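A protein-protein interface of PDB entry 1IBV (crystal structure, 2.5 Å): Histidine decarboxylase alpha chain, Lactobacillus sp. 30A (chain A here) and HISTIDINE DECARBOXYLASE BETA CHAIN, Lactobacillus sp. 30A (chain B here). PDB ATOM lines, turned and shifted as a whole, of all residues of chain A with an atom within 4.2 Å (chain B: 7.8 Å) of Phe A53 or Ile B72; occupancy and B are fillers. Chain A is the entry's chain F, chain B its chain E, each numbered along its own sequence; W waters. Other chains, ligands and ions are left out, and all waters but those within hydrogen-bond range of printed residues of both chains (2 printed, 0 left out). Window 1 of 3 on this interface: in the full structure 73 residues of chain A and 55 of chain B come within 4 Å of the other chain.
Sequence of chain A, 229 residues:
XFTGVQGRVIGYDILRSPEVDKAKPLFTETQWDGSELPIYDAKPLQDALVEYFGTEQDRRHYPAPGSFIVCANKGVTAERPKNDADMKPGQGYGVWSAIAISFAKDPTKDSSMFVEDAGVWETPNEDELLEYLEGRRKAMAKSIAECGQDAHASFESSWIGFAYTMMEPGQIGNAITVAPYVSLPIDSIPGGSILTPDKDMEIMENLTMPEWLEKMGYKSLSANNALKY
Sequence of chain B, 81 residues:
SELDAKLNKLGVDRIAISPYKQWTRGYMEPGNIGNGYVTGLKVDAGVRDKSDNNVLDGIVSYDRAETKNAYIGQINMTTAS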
ATOM      1  N   LEU A  49      13.706  30.573  26.234  1.00  0.00           N
ATOM      2  CA  LEU A  49      12.763  30.279  25.171  1.00  0.00           C
ATOM      3  C   LEU A  49      11.362  30.698  25.585  1.00  0.00           C
ATOM      4  O   LEU A  49      10.619  31.270  24.788  1.00  0.00           O
ATOM      5  CB  LEU A  49      12.785  28.790  24.827  1.00  0.00           C
ATOM      6  CG  LEU A  49      11.992  28.336  23.599  1.00  0.00           C
ATOM      7  CD1 LEU A  49      12.528  28.982  22.328  1.00  0.00           C
ATOM      8  CD2 LEU A  49      12.089  26.843  23.487  1.00  0.00           C
ATOM      9  N   VAL A  50      11.017  30.457  26.846  1.00  0.00           N
ATOM     10  CA  VAL A  50       9.698  30.822  27.341  1.00  0.00           C
ATOM     11  C   VAL A  50       9.521  32.333  27.266  1.00  0.00           C
ATOM     12  O   VAL A  50       8.450  32.828  26.933  1.00  0.00           O
ATOM     13  CB  VAL A  50       9.487  30.346  28.787  1.00  0.00           C
ATOM     14  CG1 VAL A  50       8.058  30.644  29.248  1.00  0.00           C
ATOM     15  CG2 VAL A  50       9.767  28.856  28.888  1.00  0.00           C
ATOM     16  N   GLU A  51      10.587  33.064  27.551  1.00  0.00           N
ATOM     17  CA  GLU A  51      10.533  34.514  27.511  1.00  0.00           C
ATOM     18  C   GLU A  51      10.241  35.040  26.107  1.00  0.00           C
ATOM     19  O   GLU A  51       9.571  36.057  25.946  1.00  0.00           O
ATOM     20  CB  GLU A  51      11.848  35.100  28.032  1.00  0.00           C
ATOM     21  CG  GLU A  51      12.142  34.794  29.493  1.00  0.00           C
ATOM     22  CD  GLU A  51      11.313  35.628  30.456  1.00  0.00           C
ATOM     23  OE1 GLU A  51      10.170  36.002  30.114  1.00  0.00           O
ATOM     24  OE2 GLU A  51      11.810  35.919  31.562  1.00  0.00           O
ATOM     25  N   TYR A  52      10.759  34.345  25.094  1.00  0.00           N
ATOM     26  CA  TYR A  52      10.569  34.753  23.699  1.00  0.00           C
ATOM     27  C   TYR A  52       9.230  34.290  23.117  1.00  0.00           C
ATOM     28  O   TYR A  52       8.480  35.098  22.564  1.00  0.00           O
ATOM     29  CB  TYR A  52      11.725  34.247  22.831  1.00  0.00           C
ATOM     30  CG  TYR A  52      11.753  34.855  21.446  1.00  0.00           C
ATOM     31  CD1 TYR A  52      12.090  36.192  21.265  1.00  0.00           C
ATOM     32  CD2 TYR A  52      11.410  34.101  20.328  1.00  0.00           C
ATOM     33  CE1 TYR A  52      12.081  36.767  20.009  1.00  0.00           C
ATOM     34  CE2 TYR A  52      11.398  34.663  19.071  1.00  0.00           C
ATOM     35  CZ  TYR A  52      11.733  35.999  18.918  1.00  0.00           C
ATOM     36  OH  TYR A  52      11.703  36.578  17.677  1.00  0.00           O
ATOM     37  N   PHE A  53       8.945  32.993  23.204  1.00  0.00           N
ATOM     38  CA  PHE A  53       7.684  32.463  22.693  1.00  0.00           C
ATOM     39  C   PHE A  53       6.489  32.885  23.523  1.00  0.00           C
ATOM     40  O   PHE A  53       5.397  33.081  22.996  1.00  0.00           O
ATOM     41  CB  PHE A  53       7.710  30.939  22.639  1.00  0.00           C
ATOM     42  CG  PHE A  53       8.485  30.381  21.485  1.00  0.00           C
ATOM     43  CD1 PHE A  53       8.551  29.009  21.286  1.00  0.00           C
ATOM     44  CD2 PHE A  53       9.144  31.219  20.597  1.00  0.00           C
ATOM     45  CE1 PHE A  53       9.276  28.476  20.233  1.00  0.00           C
ATOM     46  CE2 PHE A  53       9.875  30.698  19.535  1.00  0.00           C
ATOM     47  CZ  PHE A  53       9.936  29.322  19.349  1.00  0.00           C
ATOM     48  N   GLY A  54       6.704  33.072  24.815  1.00  0.00           N
ATOM     49  CA  GLY A  54       5.609  33.427  25.688  1.00  0.00           C
ATOM     50  C   GLY A  54       4.919  32.128  26.069  1.00  0.00           C
ATOM     51  O   GLY A  54       5.333  31.042  25.634  1.00  0.00           O
ATOM     52  N   ARG A  59       0.992  34.904  25.477  1.00  0.00           N
ATOM     53  CA  ARG A  59       1.654  34.658  24.200  1.00  0.00           C
ATOM     54  C   ARG A  59       2.467  35.820  23.655  1.00  0.00           C
ATOM     55  O   ARG A  59       2.017  36.968  23.640  1.00  0.00           O
ATOM     56  CB  ARG A  59       0.631  34.224  23.156  1.00  0.00           C
ATOM     57  CG  ARG A  59      -0.139  32.985  23.535  1.00  0.00           C
ATOM     58  CD  ARG A  59      -1.069  32.574  22.433  1.00  0.00           C
ATOM     59  NE  ARG A  59      -1.944  31.498  22.864  1.00  0.00           N
ATOM     60  CZ  ARG A  59      -2.709  30.792  22.047  1.00  0.00           C
ATOM     61  NH1 ARG A  59      -3.485  29.828  22.519  1.00  0.00           N
ATOM     62  NH2 ARG A  59      -2.675  31.032  20.748  1.00  0.00           N
ATOM     63  N   ARG A  60       3.661  35.495  23.171  1.00  0.00           N
ATOM     64  CA  ARG A  60       4.551  36.485  22.609  1.00  0.00           C
ATOM     65  C   ARG A  60       4.909  36.117  21.175  1.00  0.00           C
ATOM     66  O   ARG A  60       4.037  36.102  20.311  1.00  0.00           O
ATOM     67  CB  ARG A  60       5.788  36.648  23.490  1.00  0.00           C
ATOM     68  CG  ARG A  60       5.441  37.254  24.827  1.00  0.00           C
ATOM     69  CD  ARG A  60       6.583  37.204  25.807  1.00  0.00           C
ATOM     70  NE  ARG A  60       6.181  37.821  27.066  1.00  0.00           N
ATOM     71  CZ  ARG A  60       6.939  37.885  28.153  1.00  0.00           C
ATOM     72  NH1 ARG A  60       6.468  38.473  29.242  1.00  0.00           N
ATOM     73  NH2 ARG A  60       8.158  37.372  28.148  1.00  0.00           N
ATOM     74  N   HIS A  61       6.161  35.778  20.915  1.00  0.00           N
ATOM     75  CA  HIS A  61       6.570  35.449  19.560  1.00  0.00           C
ATOM     76  C   HIS A  61       6.595  33.969  19.263  1.00  0.00           C
ATOM     77  O   HIS A  61       7.591  33.417  18.804  1.00  0.00           O
ATOM     78  CB  HIS A  61       7.891  36.142  19.263  1.00  0.00           C
ATOM     79  CG  HIS A  61       7.840  37.603  19.547  1.00  0.00           C
ATOM     80  ND1 HIS A  61       7.095  38.478  18.782  1.00  0.00           N
ATOM     81  CD2 HIS A  61       8.334  38.334  20.572  1.00  0.00           C
ATOM     82  CE1 HIS A  61       7.125  39.678  19.329  1.00  0.00           C
ATOM     83  NE2 HIS A  61       7.872  39.620  20.419  1.00  0.00           N
ATOM     84  N   TYR A  62       5.470  33.323  19.533  1.00  0.00           N
ATOM     85  CA  TYR A  62       5.344  31.899  19.296  1.00  0.00           C
ATOM     86  C   TYR A  62       5.225  31.653  17.805  1.00  0.00           C
ATOM     87  O   TYR A  62       4.940  32.567  17.038  1.00  0.00           O
ATOM     88  CB  TYR A  62       4.119  31.358  20.034  1.00  0.00           C
ATOM     89  CG  TYR A  62       2.799  31.885  19.536  1.00  0.00           C
ATOM     90  CD1 TYR A  62       2.339  33.140  19.923  1.00  0.00           C
ATOM     91  CD2 TYR A  62       1.995  31.111  18.700  1.00  0.00           C
ATOM     92  CE1 TYR A  62       1.111  33.607  19.492  1.00  0.00           C
ATOM     93  CE2 TYR A  62       0.769  31.566  18.267  1.00  0.00           C
ATOM     94  CZ  TYR A  62       0.332  32.813  18.667  1.00  0.00           C
ATOM     95  OH  TYR A  62      -0.888  33.267  18.239  1.00  0.00           O
ATOM     96  N   PRO A  63       5.430  30.405  17.367  1.00  0.00           N
ATOM     97  CA  PRO A  63       5.341  30.048  15.954  1.00  0.00           C
ATOM     98  C   PRO A  63       3.973  30.334  15.375  1.00  0.00           C
ATOM     99  O   PRO A  63       2.964  30.253  16.077  1.00  0.00           O
ATOM    100  CB  PRO A  63       5.646  28.561  15.966  1.00  0.00           C
ATOM    101  CG  PRO A  63       6.553  28.424  17.124  1.00  0.00           C
ATOM    102  CD  PRO A  63       5.858  29.246  18.159  1.00  0.00           C
ATOM    103  N   GLN B  22       4.225  39.472  14.658  1.00  0.00           N
ATOM    104  CA  GLN B  22       4.281  38.735  15.926  1.00  0.00           C
ATOM    105  C   GLN B  22       4.868  37.338  15.915  1.00  0.00           C
ATOM    106  O   GLN B  22       5.762  37.045  16.703  1.00  0.00           O
ATOM    107  CB  GLN B  22       2.907  38.679  16.595  1.00  0.00           C
ATOM    108  CG  GLN B  22       2.925  38.004  17.956  1.00  0.00           C
ATOM    109  CD  GLN B  22       1.552  37.909  18.597  1.00  0.00           C
ATOM    110  OE1 GLN B  22       0.585  38.513  18.138  1.00  0.00           O
ATOM    111  NE2 GLN B  22       1.468  37.148  19.670  1.00  0.00           N
ATOM    112  N   TRP B  23       4.351  36.482  15.048  1.00  0.00           N
ATOM    113  CA  TRP B  23       4.787  35.092  14.956  1.00  0.00           C
ATOM    114  C   TRP B  23       6.152  34.779  14.343  1.00  0.00           C
ATOM    115  O   TRP B  23       6.686  35.530  13.519  1.00  0.00           O
ATOM    116  CB  TRP B  23       3.749  34.278  14.195  1.00  0.00           C
ATOM    117  CG  TRP B  23       2.373  34.439  14.676  1.00  0.00           C
ATOM    118  CD1 TRP B  23       1.938  34.339  15.956  1.00  0.00           C
ATOM    119  CD2 TRP B  23       1.221  34.704  13.877  1.00  0.00           C
ATOM    120  NE1 TRP B  23       0.578  34.521  16.009  1.00  0.00           N
ATOM    121  CE2 TRP B  23       0.112  34.747  14.744  1.00  0.00           C
ATOM    122  CE3 TRP B  23       1.015  34.912  12.509  1.00  0.00           C
ATOM    123  CZ2 TRP B  23      -1.182  34.983  14.293  1.00  0.00           C
ATOM    124  CZ3 TRP B  23      -0.267  35.145  12.061  1.00  0.00           C
ATOM    125  CH2 TRP B  23      -1.351  35.186  12.949  1.00  0.00           C
ATOM    126  N   THR B  24       6.701  33.650  14.768  1.00  0.00           N
ATOM    127  CA  THR B  24       7.959  33.149  14.266  1.00  0.00           C
ATOM    128  C   THR B  24       7.544  32.147  13.199  1.00  0.00           C
ATOM    129  O   THR B  24       6.364  31.807  13.100  1.00  0.00           O
ATOM    130  CB  THR B  24       8.744  32.427  15.369  1.00  0.00           C
ATOM    131  OG1 THR B  24       7.833  31.894  16.334  1.00  0.00           O
ATOM    132  CG2 THR B  24       9.710  33.368  16.052  1.00  0.00           C
ATOM    133  N   ARG B  25       8.489  31.692  12.387  1.00  0.00           N
ATOM    134  CA  ARG B  25       8.193  30.719  11.349  1.00  0.00           C
ATOM    135  C   ARG B  25       9.306  29.696  11.371  1.00  0.00           C
ATOM    136  O   ARG B  25      10.355  29.933  11.962  1.00  0.00           O
ATOM    137  CB  ARG B  25       8.121  31.390   9.978  1.00  0.00           C
ATOM    138  CG  ARG B  25       7.021  32.423   9.849  1.00  0.00           C
ATOM    139  CD  ARG B  25       6.969  33.022   8.457  1.00  0.00           C
ATOM    140  NE  ARG B  25       6.363  32.115   7.484  1.00  0.00           N
ATOM    141  CZ  ARG B  25       6.745  32.020   6.214  1.00  0.00           C
ATOM    142  NH1 ARG B  25       6.130  31.173   5.408  1.00  0.00           N
ATOM    143  NH2 ARG B  25       7.755  32.752   5.761  1.00  0.00           N
ATOM    144  N   VAL B  38      17.494  30.083  13.860  1.00  0.00           N
ATOM    145  CA  VAL B  38      17.648  30.305  15.289  1.00  0.00           C
ATOM    146  C   VAL B  38      16.970  29.130  15.979  1.00  0.00           C
ATOM    147  O   VAL B  38      15.969  28.605  15.489  1.00  0.00           O
ATOM    148  CB  VAL B  38      16.982  31.608  15.726  1.00  0.00           C
ATOM    149  CG1 VAL B  38      17.065  31.762  17.233  1.00  0.00           C
ATOM    150  CG2 VAL B  38      17.652  32.779  15.053  1.00  0.00           C
ATOM    151  N   THR B  39      17.533  28.688  17.094  1.00  0.00           N
ATOM    152  CA  THR B  39      16.967  27.561  17.811  1.00  0.00           C
ATOM    153  C   THR B  39      16.918  27.821  19.312  1.00  0.00           C
ATOM    154  O   THR B  39      17.391  28.853  19.792  1.00  0.00           O
ATOM    155  CB  THR B  39      17.762  26.295  17.511  1.00  0.00           C
ATOM    156  OG1 THR B  39      17.059  25.160  18.009  1.00  0.00           O
ATOM    157  CG2 THR B  39      19.115  26.354  18.154  1.00  0.00           C
ATOM    158  N   GLY B  40      16.353  26.872  20.048  1.00  0.00           N
ATOM    159  CA  GLY B  40      16.235  27.003  21.486  1.00  0.00           C
ATOM    160  C   GLY B  40      16.006  25.645  22.106  1.00  0.00           C
ATOM    161  O   GLY B  40      15.893  24.653  21.379  1.00  0.00           O
ATOM    162  N   LYS B  42      13.602  23.206  24.585  1.00  0.00           N
ATOM    163  CA  LYS B  42      12.309  23.017  25.225  1.00  0.00           C
ATOM    164  C   LYS B  42      12.091  21.577  25.629  1.00  0.00           C
ATOM    165  O   LYS B  42      12.168  20.669  24.809  1.00  0.00           O
ATOM    166  CB  LYS B  42      11.153  23.444  24.325  1.00  0.00           C
ATOM    167  CG  LYS B  42       9.787  23.182  24.964  1.00  0.00           C
ATOM    168  CD  LYS B  42       8.658  23.336  23.964  1.00  0.00           C
ATOM    169  CE  LYS B  42       7.371  22.677  24.444  1.00  0.00           C
ATOM    170  NZ  LYS B  42       6.689  23.447  25.517  1.00  0.00           N
ATOM    171  N   ASP B  44       9.294  19.458  28.064  1.00  0.00           N
ATOM    172  CA  ASP B  44       8.057  19.527  28.818  1.00  0.00           C
ATOM    173  C   ASP B  44       7.334  18.210  28.768  1.00  0.00           C
ATOM    174  O   ASP B  44       7.616  17.375  27.911  1.00  0.00           O
ATOM    175  CB  ASP B  44       7.146  20.625  28.285  1.00  0.00           C
ATOM    176  CG  ASP B  44       7.593  21.999  28.716  1.00  0.00           C
ATOM    177  OD1 ASP B  44       7.963  22.798  27.844  1.00  0.00           O
ATOM    178  OD2 ASP B  44       7.599  22.273  29.934  1.00  0.00           O
ATOM    179  N   TYR B  62       0.699  14.849  23.931  1.00  0.00           N
ATOM    180  CA  TYR B  62       1.746  15.488  23.129  1.00  0.00           C
ATOM    181  C   TYR B  62       1.282  16.866  22.657  1.00  0.00           C
ATOM    182  O   TYR B  62       1.978  17.534  21.913  1.00  0.00           O
ATOM    183  CB  TYR B  62       2.094  14.582  21.938  1.00  0.00           C
ATOM    184  CG  TYR B  62       2.876  15.223  20.815  1.00  0.00           C
ATOM    185  CD1 TYR B  62       4.222  15.555  20.972  1.00  0.00           C
ATOM    186  CD2 TYR B  62       2.267  15.480  19.586  1.00  0.00           C
ATOM    187  CE1 TYR B  62       4.951  16.123  19.930  1.00  0.00           C
ATOM    188  CE2 TYR B  62       2.977  16.045  18.535  1.00  0.00           C
ATOM    189  CZ  TYR B  62       4.322  16.366  18.708  1.00  0.00           C
ATOM    190  OH  TYR B  62       5.039  16.905  17.655  1.00  0.00           O
ATOM    191  N   ASP B  63       0.134  17.308  23.153  1.00  0.00           N
ATOM    192  CA  ASP B  63      -0.427  18.596  22.790  1.00  0.00           C
ATOM    193  C   ASP B  63      -0.420  19.449  24.048  1.00  0.00           C
ATOM    194  O   ASP B  63      -0.197  20.663  23.988  1.00  0.00           O
ATOM    195  CB  ASP B  63      -1.852  18.422  22.272  1.00  0.00           C
ATOM    196  CG  ASP B  63      -2.379  19.662  21.590  1.00  0.00           C
ATOM    197  OD1 ASP B  63      -2.215  19.778  20.352  1.00  0.00           O
ATOM    198  OD2 ASP B  63      -2.952  20.523  22.288  1.00  0.00           O
ATOM    199  N   ALA B  65       1.711  19.090  26.234  1.00  0.00           N
ATOM    200  CA  ALA B  65       3.133  19.336  26.423  1.00  0.00           C
ATOM    201  C   ALA B  65       3.585  20.492  25.547  1.00  0.00           C
ATOM    202  O   ALA B  65       4.382  21.314  25.979  1.00  0.00           O
ATOM    203  CB  ALA B  65       3.940  18.093  26.103  1.00  0.00           C
ATOM    204  N   GLU B  66       3.063  20.561  24.323  1.00  0.00           N
ATOM    205  CA  GLU B  66       3.426  21.637  23.399  1.00  0.00           C
ATOM    206  C   GLU B  66       2.895  22.975  23.879  1.00  0.00           C
ATOM    207  O   GLU B  66       3.479  24.023  23.601  1.00  0.00           O
ATOM    208  CB  GLU B  66       2.864  21.376  21.995  1.00  0.00           C
ATOM    209  CG  GLU B  66       3.468  20.188  21.279  1.00  0.00           C
ATOM    210  CD  GLU B  66       2.934  20.030  19.877  1.00  0.00           C
ATOM    211  OE1 GLU B  66       3.763  19.902  18.953  1.00  0.00           O
ATOM    212  OE2 GLU B  66       1.690  20.033  19.699  1.00  0.00           O
ATOM    213  N   THR B  67       1.763  22.937  24.570  1.00  0.00           N
ATOM    214  CA  THR B  67       1.125  24.143  25.073  1.00  0.00           C
ATOM    215  C   THR B  67       1.581  24.549  26.472  1.00  0.00           C
ATOM    216  O   THR B  67       1.225  25.625  26.956  1.00  0.00           O
ATOM    217  CB  THR B  67      -0.391  23.968  25.076  1.00  0.00           C
ATOM    218  OG1 THR B  67      -0.720  22.778  25.796  1.00  0.00           O
ATOM    219  CG2 THR B  67      -0.908  23.822  23.654  1.00  0.00           C
ATOM    220  N   LYS B  68       2.388  23.703  27.104  1.00  0.00           N
ATOM    221  CA  LYS B  68       2.866  23.983  28.448  1.00  0.00           C
ATOM    222  C   LYS B  68       4.134  24.814  28.385  1.00  0.00           C
ATOM    223  O   LYS B  68       4.988  24.590  27.534  1.00  0.00           O
ATOM    224  CB  LYS B  68       3.113  22.686  29.213  1.00  0.00           C
ATOM    225  CG  LYS B  68       3.322  22.891  30.707  1.00  0.00           C
ATOM    226  CD  LYS B  68       3.508  21.571  31.442  1.00  0.00           C
ATOM    227  CE  LYS B  68       3.841  21.802  32.904  1.00  0.00           C
ATOM    228  NZ  LYS B  68       3.836  20.530  33.676  1.00  0.00           N
ATOM    229  N   ASN B  69       4.272  25.752  29.314  1.00  0.00           N
ATOM    230  CA  ASN B  69       5.429  26.638  29.342  1.00  0.00           C
ATOM    231  C   ASN B  69       5.623  27.329  27.987  1.00  0.00           C
ATOM    232  O   ASN B  69       4.744  28.078  27.565  1.00  0.00           O
ATOM    233  CB  ASN B  69       6.689  25.902  29.830  1.00  0.00           C
ATOM    234  CG  ASN B  69       6.683  25.674  31.347  1.00  0.00           C
ATOM    235  OD1 ASN B  69       6.304  26.559  32.121  1.00  0.00           O
ATOM    236  ND2 ASN B  69       7.092  24.488  31.770  1.00  0.00           N
ATOM    237  N   ALA B  70       6.736  27.070  27.297  1.00  0.00           N
ATOM    238  CA  ALA B  70       6.991  27.705  26.000  1.00  0.00           C
ATOM    239  C   ALA B  70       5.966  27.217  25.003  1.00  0.00           C
ATOM    240  O   ALA B  70       5.911  26.037  24.673  1.00  0.00           O
ATOM    241  CB  ALA B  70       8.389  27.404  25.512  1.00  0.00           C
ATOM    242  N   TYR B  71       5.165  28.141  24.502  1.00  0.00           N
ATOM    243  CA  TYR B  71       4.119  27.788  23.569  1.00  0.00           C
ATOM    244  C   TYR B  71       4.551  27.508  22.136  1.00  0.00           C
ATOM    245  O   TYR B  71       5.264  28.295  21.509  1.00  0.00           O
ATOM    246  CB  TYR B  71       3.045  28.869  23.567  1.00  0.00           C
ATOM    247  CG  TYR B  71       1.806  28.521  22.777  1.00  0.00           C
ATOM    248  CD1 TYR B  71       0.842  27.665  23.302  1.00  0.00           C
ATOM    249  CD2 TYR B  71       1.574  29.082  21.526  1.00  0.00           C
ATOM    250  CE1 TYR B  71      -0.324  27.379  22.604  1.00  0.00           C
ATOM    251  CE2 TYR B  71       0.412  28.803  20.816  1.00  0.00           C
ATOM    252  CZ  TYR B  71      -0.534  27.953  21.361  1.00  0.00           C
ATOM    253  OH  TYR B  71      -1.691  27.677  20.664  1.00  0.00           O
ATOM    254  N   ILE B  72       4.139  26.345  21.654  1.00  0.00           N
ATOM    255  CA  ILE B  72       4.367  25.917  20.288  1.00  0.00           C
ATOM    256  C   ILE B  72       3.108  25.120  19.963  1.00  0.00           C
ATOM    257  O   ILE B  72       3.128  24.126  19.243  1.00  0.00           O
ATOM    258  CB  ILE B  72       5.628  25.047  20.120  1.00  0.00           C
ATOM    259  CG1 ILE B  72       5.539  23.786  20.964  1.00  0.00           C
ATOM    260  CG2 ILE B  72       6.875  25.840  20.463  1.00  0.00           C
ATOM    261  CD1 ILE B  72       6.618  22.793  20.646  1.00  0.00           C
ATOM    262  N   GLY B  73       2.000  25.638  20.475  1.00  0.00           N
ATOM    263  CA  GLY B  73       0.701  25.021  20.318  1.00  0.00           C
ATOM    264  C   GLY B  73       0.251  24.403  19.009  1.00  0.00           C
ATOM    265  O   GLY B  73       0.215  23.170  18.877  1.00  0.00           O
ATOM    266  N   GLN B  74      -0.158  25.234  18.064  1.00  0.00           N
ATOM    267  CA  GLN B  74      -0.668  24.716  16.804  1.00  0.00           C
ATOM    268  C   GLN B  74       0.383  24.673  15.709  1.00  0.00           C
ATOM    269  O   GLN B  74       0.216  25.252  14.646  1.00  0.00           O
ATOM    270  CB  GLN B  74      -1.884  25.538  16.388  1.00  0.00           C
ATOM    271  CG  GLN B  74      -2.986  25.521  17.425  1.00  0.00           C
ATOM    272  CD  GLN B  74      -4.137  26.405  17.040  1.00  0.00           C
ATOM    273  OE1 GLN B  74      -3.973  27.613  16.894  1.00  0.00           O
ATOM    274  NE2 GLN B  74      -5.302  25.809  16.829  1.00  0.00           N
ATOM    275  N   ILE B  75       1.429  23.906  15.965  1.00  0.00           N
ATOM    276  CA  ILE B  75       2.552  23.770  15.061  1.00  0.00           C
ATOM    277  C   ILE B  75       2.595  22.429  14.350  1.00  0.00           C
ATOM    278  O   ILE B  75       2.173  21.418  14.897  1.00  0.00           O
ATOM    279  CB  ILE B  75       3.862  23.985  15.861  1.00  0.00           C
ATOM    280  CG1 ILE B  75       4.242  25.451  15.814  1.00  0.00           C
ATOM    281  CG2 ILE B  75       4.985  23.084  15.396  1.00  0.00           C
ATOM    282  CD1 ILE B  75       3.144  26.361  16.306  1.00  0.00           C
ATOM    283  N   ASN B  76       3.061  22.433  13.107  1.00  0.00           N
ATOM    284  CA  ASN B  76       3.213  21.195  12.350  1.00  0.00           C
ATOM    285  C   ASN B  76       4.660  20.834  12.625  1.00  0.00           C
ATOM    286  O   ASN B  76       5.570  21.441  12.062  1.00  0.00           O
ATOM    287  CB  ASN B  76       3.020  21.429  10.854  1.00  0.00           C
ATOM    288  CG  ASN B  76       1.577  21.597  10.480  1.00  0.00           C
ATOM    289  OD1 ASN B  76       0.797  20.638  10.501  1.00  0.00           O
ATOM    290  ND2 ASN B  76       1.199  22.820  10.140  1.00  0.00           N
ATOM    291  N   MET B  77       4.880  19.894  13.531  1.00  0.00           N
ATOM    292  CA  MET B  77       6.241  19.523  13.874  1.00  0.00           C
ATOM    293  C   MET B  77       6.874  18.510  12.930  1.00  0.00           C
ATOM    294  O   MET B  77       6.352  17.415  12.733  1.00  0.00           O
ATOM    295  CB  MET B  77       6.298  19.013  15.314  1.00  0.00           C
ATOM    296  CG  MET B  77       7.718  18.877  15.846  1.00  0.00           C
ATOM    297  SD  MET B  77       7.796  18.243  17.525  1.00  0.00           S
ATOM    298  CE  MET B  77       7.089  19.600  18.387  1.00  0.00           C
HETATM  299  O   HOH W   1      -4.529  29.194  19.889  1.00  0.00           O
HETATM  300  O   HOH W   2      -0.543  37.358  21.813  1.00  0.00           O
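Water W1 lies within hydrogen-bond range of NH2 of Arg A59 (2.7 Å), OH of Tyr B71 (3.3 Å) and OE1 of Gln B74 (3.4 Å). Water W2 lies within hydrogen-bond range of the side-chain amide nitrogen (NE2) of Gln B22 and the backbone carbonyl oxygen (O) of Arg A59.
Of the 11 printed residues of chain A, 10 touch a printed residue of chain B. Printed residues of chain A that touch a printed residue of chain B: Leu A49, Val A50, Tyr A52, Phe A53, Gly A54, Arg A59, Arg A60, His A61, Tyr A62 and Pro A63. Hydrophobic or aromatic side chains of chain A within 4 Å of the printed part of chain B: Leu A49, Val A50, Tyr A52, Phe A53, His A61, Tyr A62 and Pro A63. Among the printed residues, no Asp or Glu carboxylate lies within 4 Å of a Lys or Arg side-chain nitrogen of the other chain.
The indole nitrogen of Trp B23 sits at hydrogen-bond distance from the side-chain hydroxyl of Tyr A62. The backbone carbonyl oxygen (O) of His A61 is in hydrogen-bond range of the side-chain hydroxyl (OG1) of Thr B24 (2.9 Å). The side-chain amide nitrogen (NE2) of Gln B22 lies within hydrogen-bond range of the backbone carbonyl oxygen (O) of Arg A60. ND1 of His A61 sits at hydrogen-bond distance from O of Gln B22, 2.9 Å away. The guanidinium group (NH1) of Arg A59 sits at hydrogen-bond distance from the side-chain hydroxyl (OH) of Tyr B71, at 3.4 Å. The backbone NH (N) of Tyr B71 lies within hydrogen-bond range of the backbone carbonyl oxygen (O) of Gly A54 (3.1 Å). The side-chain hydroxyl of Thr B24 lies close to the backbone carbonyl oxygen of Tyr A62. The side-chain hydroxyl of Thr B24 sits close to the backbone nitrogen of Pro A63 (3.0 Å).
Printed residues of chain B within 4 Å of Phe A53: Thr B24 (3.98 Å), Tyr B71 (3.4 Å) and Ile B72 (3.6 Å). Of chain B, only Asn B69, Ala B70 and Tyr B71 come within 4 Å of Gly A54. Printed residues of chain B within 4 Å of Tyr A62: Gln B22, Trp B23, Thr B24 and Tyr B71. Of the printed residues of chain A, Lys B42 touches Leu A49 (3.6 Å). Ile B72 touches just one residue of chain A: Phe A53 (3.6 Å). The nearest printed residue of chain B that does not touch Phe A53 is Ala B70 (4.5 Å). The nearest printed residue of chain A that does not touch Ile B72 is Pro A63 (4.2 Å).
Among the printed residues, merely in contact across the chains: Leu A49 with Lys B42 (3.6 Å), Val A50 with Ala B70 (3.9 Å), Tyr A52 with Thr B24 (3.7 Å), Phe A53 with Thr B24 (3.98 Å), Phe A53 with Tyr B71 (3.4 Å), Phe A53 with Ile B72 (3.6 Å), Gly A54 with Asn B69 (3.6 Å), Gly A54 with Ala B70 (3.7 Å), Tyr A62 with Gln B22 (3.6 Å), Tyr A62 with Tyr B71 (3.5 Å), Pro A63 with Tyr B71 (3.5 Å) and Pro A63 with Ile B75 (3.3 Å).
O of Tyr A52 is in hydrogen-bond range of N of His A61 (2.9 Å). The backbone carbonyl oxygen of Phe A53 is in hydrogen-bond range of the backbone NH of Tyr A62, 3.5 Å away. NH2 of Arg A60 is in salt-bridge range of OE1 of Glu A51, 3.1 Å away. O of Ala B65 is in hydrogen-bond range of NZ of Lys B42, at 3.2 Å.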
